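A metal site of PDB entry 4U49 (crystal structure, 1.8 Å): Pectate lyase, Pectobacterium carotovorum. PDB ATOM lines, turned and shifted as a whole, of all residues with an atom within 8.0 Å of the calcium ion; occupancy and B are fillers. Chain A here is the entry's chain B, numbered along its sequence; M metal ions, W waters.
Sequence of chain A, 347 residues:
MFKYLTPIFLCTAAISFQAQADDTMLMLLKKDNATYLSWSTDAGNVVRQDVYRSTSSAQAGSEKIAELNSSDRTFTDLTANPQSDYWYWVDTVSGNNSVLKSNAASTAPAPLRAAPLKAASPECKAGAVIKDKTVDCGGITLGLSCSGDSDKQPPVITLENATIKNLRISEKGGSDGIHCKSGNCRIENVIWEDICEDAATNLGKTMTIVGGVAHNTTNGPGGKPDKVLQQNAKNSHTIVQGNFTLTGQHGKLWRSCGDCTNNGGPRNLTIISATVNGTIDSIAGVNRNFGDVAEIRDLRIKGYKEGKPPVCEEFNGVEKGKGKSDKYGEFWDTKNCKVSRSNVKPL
The backbone carbonyl oxygen (O) of Asn 216 lies within hydrogen-bond range of the backbone NH (N) of Gln 249 (2.8 Å). The backbone NH (N) of Ile 195 is in hydrogen-bond range of the backbone carbonyl oxygen (O) of His 215. SG of Cys 196 forms a disulfide with SG of Cys 146 (2.0 Å). The side-chain hydroxyl (OG1) of Thr 217 lies within hydrogen-bond range of the backbone NH (N) of Gly 220, 2.9 Å away.
Thr 217 touches the calcium ion. Five residues have an atom within 4 Å of the calcium ion: Asp 194, Ile 195, Asn 216, Thr 217 and Pro 221.
The side-chain amide oxygen (OD1) of Asn 216 binds the calcium ion (2.4 Å). O of Pro 221 binds the calcium ion (2.5 Å). Water W2 binds the calcium ion, at 2.5 Å. The side-chain carboxylate (OD2) of Asp 194 is bound to the calcium ion (2.5 Å). The calcium ion is bound by O of Ile 195 (2.6 Å).
Water W1 bridges the backbone carbonyl oxygen (O) of Cys 196 (2.8 Å) and the side-chain amide nitrogen (ND2) of Asn 216 (3.3 Å).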
ATOM      1  N   CYS A 146      13.389  13.461  -9.920  1.00  0.00           N
ATOM      2  CA  CYS A 146      13.311  12.927  -8.564  1.00  0.00           C
ATOM      3  C   CYS A 146      13.578  14.009  -7.524  1.00  0.00           C
ATOM      4  O   CYS A 146      14.714  14.446  -7.349  1.00  0.00           O
ATOM      5  CB  CYS A 146      14.297  11.767  -8.376  1.00  0.00           C
ATOM      6  SG  CYS A 146      14.171  10.985  -6.757  1.00  0.00           S
ATOM      7  N   GLU A 171      17.586   6.111 -13.264  1.00  0.00           N
ATOM      8  CA  GLU A 171      18.039   6.272 -11.890  1.00  0.00           C
ATOM      9  C   GLU A 171      17.853   7.709 -11.381  1.00  0.00           C
ATOM     10  O   GLU A 171      17.820   7.938 -10.178  1.00  0.00           O
ATOM     11  CB  GLU A 171      19.511   5.862 -11.758  1.00  0.00           C
ATOM     12  CG  GLU A 171      20.493   6.770 -12.469  1.00  0.00           C
ATOM     13  CD  GLU A 171      21.940   6.435 -12.131  1.00  0.00           C
ATOM     14  OE1 GLU A 171      22.164   5.478 -11.365  1.00  0.00           O
ATOM     15  OE2 GLU A 171      22.846   7.132 -12.631  1.00  0.00           O
ATOM     16  N   GLU A 193      16.087   1.379 -11.785  1.00  0.00           N
ATOM     17  CA  GLU A 193      17.513   1.625 -11.590  1.00  0.00           C
ATOM     18  C   GLU A 193      17.785   2.302 -10.253  1.00  0.00           C
ATOM     19  O   GLU A 193      18.848   2.104  -9.661  1.00  0.00           O
ATOM     20  CB  GLU A 193      18.075   2.469 -12.733  1.00  0.00           C
ATOM     21  CG  GLU A 193      18.163   1.723 -14.044  1.00  0.00           C
ATOM     22  CD  GLU A 193      18.922   2.507 -15.102  1.00  0.00           C
ATOM     23  OE1 GLU A 193      18.789   3.751 -15.122  1.00  0.00           O
ATOM     24  OE2 GLU A 193      19.650   1.881 -15.898  1.00  0.00           O
ATOM     25  N   ASP A 194      16.835   3.092  -9.782  1.00  0.00           N
ATOM     26  CA  ASP A 194      16.949   3.768  -8.496  1.00  0.00           C
ATOM     27  C   ASP A 194      15.584   4.290  -8.065  1.00  0.00           C
ATOM     28  O   ASP A 194      15.073   5.262  -8.632  1.00  0.00           O
ATOM     29  CB  ASP A 194      17.955   4.908  -8.577  1.00  0.00           C
ATOM     30  CG  ASP A 194      18.448   5.345  -7.212  1.00  0.00           C
ATOM     31  OD1 ASP A 194      19.501   4.843  -6.769  1.00  0.00           O
ATOM     32  OD2 ASP A 194      17.772   6.192  -6.583  1.00  0.00           O
ATOM     33  N   ILE A 195      14.998   3.649  -7.054  1.00  0.00           N
ATOM     34  CA  ILE A 195      13.689   4.067  -6.554  1.00  0.00           C
ATOM     35  C   ILE A 195      13.767   5.477  -5.982  1.00  0.00           C
ATOM     36  O   ILE A 195      14.612   5.774  -5.151  1.00  0.00           O
ATOM     37  CB  ILE A 195      13.163   3.122  -5.468  1.00  0.00           C
ATOM     38  CG1 ILE A 195      13.029   1.700  -6.011  1.00  0.00           C
ATOM     39  CG2 ILE A 195      11.808   3.622  -4.948  1.00  0.00           C
ATOM     40  CD1 ILE A 195      12.597   0.687  -4.981  1.00  0.00           C
ATOM     41  N   CYS A 196      12.873   6.339  -6.445  1.00  0.00           N
ATOM     42  CA  CYS A 196      12.790   7.694  -5.930  1.00  0.00           C
ATOM     43  C   CYS A 196      11.837   7.728  -4.736  1.00  0.00           C
ATOM     44  O   CYS A 196      12.254   7.506  -3.602  1.00  0.00           O
ATOM     45  CB  CYS A 196      12.331   8.659  -7.020  1.00  0.00           C
ATOM     46  SG  CYS A 196      12.239  10.386  -6.503  1.00  0.00           S
ATOM     47  N   GLU A 197      10.567   8.001  -4.996  1.00  0.00           N
ATOM     48  CA  GLU A 197       9.555   8.011  -3.937  1.00  0.00           C
ATOM     49  C   GLU A 197       9.032   6.605  -3.687  1.00  0.00           C
ATOM     50  O   GLU A 197       9.349   5.990  -2.663  1.00  0.00           O
ATOM     51  CB  GLU A 197       8.405   8.955  -4.298  1.00  0.00           C
ATOM     52  CG  GLU A 197       7.391   9.153  -3.188  1.00  0.00           C
ATOM     53  CD  GLU A 197       6.338  10.192  -3.549  1.00  0.00           C
ATOM     54  OE1 GLU A 197       6.511  10.877  -4.577  1.00  0.00           O
ATOM     55  OE2 GLU A 197       5.350  10.321  -2.795  1.00  0.00           O
ATOM     56  N   HIS A 215      16.362  -1.377  -7.543  1.00  0.00           N
ATOM     57  CA  HIS A 215      17.547  -0.969  -6.812  1.00  0.00           C
ATOM     58  C   HIS A 215      17.269   0.295  -6.008  1.00  0.00           C
ATOM     59  O   HIS A 215      16.485   1.141  -6.431  1.00  0.00           O
ATOM     60  CB  HIS A 215      18.718  -0.738  -7.764  1.00  0.00           C
ATOM     61  CG  HIS A 215      19.908  -0.097  -7.117  1.00  0.00           C
ATOM     62  ND1 HIS A 215      20.792  -0.787  -6.326  1.00  0.00           N
ATOM     63  CD2 HIS A 215      20.344   1.189  -7.141  1.00  0.00           C
ATOM     64  CE1 HIS A 215      21.726   0.030  -5.890  1.00  0.00           C
ATOM     65  NE2 HIS A 215      21.476   1.241  -6.372  1.00  0.00           N
ATOM     66  N   ASN A 216      17.902   0.401  -4.842  1.00  0.00           N
ATOM     67  CA  ASN A 216      17.814   1.616  -4.062  1.00  0.00           C
ATOM     68  C   ASN A 216      19.067   1.821  -3.233  1.00  0.00           C
ATOM     69  O   ASN A 216      19.745   0.855  -2.865  1.00  0.00           O
ATOM     70  CB  ASN A 216      16.584   1.610  -3.155  1.00  0.00           C
ATOM     71  CG  ASN A 216      16.202   2.987  -2.681  1.00  0.00           C
ATOM     72  OD1 ASN A 216      16.679   3.991  -3.207  1.00  0.00           O
ATOM     73  ND2 ASN A 216      15.344   3.056  -1.662  1.00  0.00           N
ATOM     74  N   THR A 217      19.374   3.080  -2.956  1.00  0.00           N
ATOM     75  CA  THR A 217      20.497   3.427  -2.107  1.00  0.00           C
ATOM     76  C   THR A 217      20.019   4.295  -0.944  1.00  0.00           C
ATOM     77  O   THR A 217      19.021   5.007  -1.064  1.00  0.00           O
ATOM     78  CB  THR A 217      21.597   4.188  -2.884  1.00  0.00           C
ATOM     79  OG1 THR A 217      21.014   5.342  -3.504  1.00  0.00           O
ATOM     80  CG2 THR A 217      22.201   3.296  -3.951  1.00  0.00           C
ATOM     81  N   THR A 218      20.724   4.228   0.172  1.00  0.00           N
ATOM     82  CA  THR A 218      20.383   5.025   1.337  1.00  0.00           C
ATOM     83  C   THR A 218      20.931   6.441   1.212  1.00  0.00           C
ATOM     84  O   THR A 218      20.668   7.301   2.046  1.00  0.00           O
ATOM     85  CB  THR A 218      20.910   4.386   2.635  1.00  0.00           C
ATOM     86  OG1 THR A 218      20.759   5.320   3.720  1.00  0.00           O
ATOM     87  CG2 THR A 218      22.382   4.032   2.492  1.00  0.00           C
ATOM     88  N   ASN A 219      21.672   6.669   0.134  1.00  0.00           N
ATOM     89  CA  ASN A 219      22.382   7.932  -0.047  1.00  0.00           C
ATOM     90  C   ASN A 219      22.031   8.626  -1.365  1.00  0.00           C
ATOM     91  O   ASN A 219      22.440   9.771  -1.595  1.00  0.00           O
ATOM     92  CB  ASN A 219      23.893   7.691   0.012  1.00  0.00           C
ATOM     93  CG  ASN A 219      24.304   6.400  -0.659  1.00  0.00           C
ATOM     94  OD1 ASN A 219      24.216   5.317  -0.067  1.00  0.00           O
ATOM     95  ND2 ASN A 219      24.750   6.491  -1.901  1.00  0.00           N
ATOM     96  N   GLY A 220      21.285   7.943  -2.224  1.00  0.00           N
ATOM     97  CA  GLY A 220      20.992   8.455  -3.549  1.00  0.00           C
ATOM     98  C   GLY A 220      19.693   9.227  -3.672  1.00  0.00           C
ATOM     99  O   GLY A 220      19.155   9.722  -2.674  1.00  0.00           O
ATOM    100  N   PRO A 221      19.176   9.339  -4.911  1.00  0.00           N
ATOM    101  CA  PRO A 221      17.977  10.095  -5.268  1.00  0.00           C
ATOM    102  C   PRO A 221      16.721   9.617  -4.537  1.00  0.00           C
ATOM    103  O   PRO A 221      16.294   8.482  -4.720  1.00  0.00           O
ATOM    104  CB  PRO A 221      17.837   9.855  -6.776  1.00  0.00           C
ATOM    105  CG  PRO A 221      19.207   9.486  -7.231  1.00  0.00           C
ATOM    106  CD  PRO A 221      19.800   8.715  -6.088  1.00  0.00           C
ATOM    107  N   GLY A 222      16.138  10.494  -3.720  1.00  0.00           N
ATOM    108  CA  GLY A 222      14.923  10.169  -2.993  1.00  0.00           C
ATOM    109  C   GLY A 222      15.112  10.169  -1.491  1.00  0.00           C
ATOM    110  O   GLY A 222      14.180   9.870  -0.741  1.00  0.00           O
ATOM    111  N   GLY A 223      16.316  10.500  -1.050  1.00  0.00           N
ATOM    112  CA  GLY A 223      16.623  10.524   0.371  1.00  0.00           C
ATOM    113  C   GLY A 223      16.754   9.139   0.952  1.00  0.00           C
ATOM    114  O   GLY A 223      17.106   8.186   0.257  1.00  0.00           O
ATOM    115  N   LYS A 224      16.472   9.017   2.246  1.00  0.00           N
ATOM    116  CA  LYS A 224      16.527   7.718   2.927  1.00  0.00           C
ATOM    117  C   LYS A 224      15.485   6.769   2.331  1.00  0.00           C
ATOM    118  O   LYS A 224      14.368   7.183   2.019  1.00  0.00           O
ATOM    119  CB  LYS A 224      16.298   7.896   4.428  1.00  0.00           C
ATOM    120  N   PRO A 225      15.851   5.489   2.178  1.00  0.00           N
ATOM    121  CA  PRO A 225      14.946   4.499   1.588  1.00  0.00           C
ATOM    122  C   PRO A 225      13.681   4.348   2.402  1.00  0.00           C
ATOM    123  O   PRO A 225      13.735   3.892   3.551  1.00  0.00           O
ATOM    124  CB  PRO A 225      15.768   3.195   1.616  1.00  0.00           C
ATOM    125  CG  PRO A 225      17.181   3.618   1.828  1.00  0.00           C
ATOM    126  CD  PRO A 225      17.106   4.875   2.647  1.00  0.00           C
ATOM    127  N   ASP A 226      12.544   4.739   1.838  1.00  0.00           N
ATOM    128  CA  ASP A 226      11.287   4.627   2.560  1.00  0.00           C
ATOM    129  C   ASP A 226      10.600   3.326   2.169  1.00  0.00           C
ATOM    130  O   ASP A 226      10.672   2.336   2.886  1.00  0.00           O
ATOM    131  CB  ASP A 226      10.386   5.834   2.271  1.00  0.00           C
ATOM    132  CG  ASP A 226       9.196   5.916   3.225  1.00  0.00           C
ATOM    133  OD1 ASP A 226       8.714   4.865   3.702  1.00  0.00           O
ATOM    134  OD2 ASP A 226       8.737   7.040   3.498  1.00  0.00           O
ATOM    135  N   GLN A 249      20.085  -1.029  -0.788  1.00  0.00           N
ATOM    136  CA  GLN A 249      19.567  -0.804   0.559  1.00  0.00           C
ATOM    137  C   GLN A 249      18.141  -0.268   0.520  1.00  0.00           C
ATOM    138  O   GLN A 249      17.871   0.765  -0.077  1.00  0.00           O
ATOM    139  CB  GLN A 249      20.482   0.159   1.328  1.00  0.00           C
ATOM    140  CG  GLN A 249      21.927  -0.297   1.451  1.00  0.00           C
ATOM    141  CD  GLN A 249      22.731  -0.047   0.188  1.00  0.00           C
ATOM    142  OE1 GLN A 249      22.641   1.027  -0.419  1.00  0.00           O
ATOM    143  NE2 GLN A 249      23.511  -1.034  -0.235  1.00  0.00           N
ATOM    144  N   HIS A 250      17.229  -0.984   1.172  1.00  0.00           N
ATOM    145  CA  HIS A 250      15.802  -0.658   1.111  1.00  0.00           C
ATOM    146  C   HIS A 250      15.199  -0.406   2.482  1.00  0.00           C
ATOM    147  O   HIS A 250      15.758  -0.785   3.507  1.00  0.00           O
ATOM    148  CB  HIS A 250      15.032  -1.773   0.410  1.00  0.00           C
ATOM    149  CG  HIS A 250      15.319  -1.879  -1.051  1.00  0.00           C
ATOM    150  ND1 HIS A 250      14.577  -1.205  -2.001  1.00  0.00           N
ATOM    151  CD2 HIS A 250      16.272  -2.561  -1.731  1.00  0.00           C
ATOM    152  CE1 HIS A 250      15.052  -1.476  -3.204  1.00  0.00           C
ATOM    153  NE2 HIS A 250      16.086  -2.297  -3.069  1.00  0.00           N
HETATM  154 CA    CA M   1      17.024   6.193  -4.152  1.00  0.00          CA
HETATM  155  O   HOH W   1      14.401   6.095  -2.370  1.00  0.00           O
HETATM  156  O   HOH W   2      17.117   7.006  -1.753  1.00  0.00           O
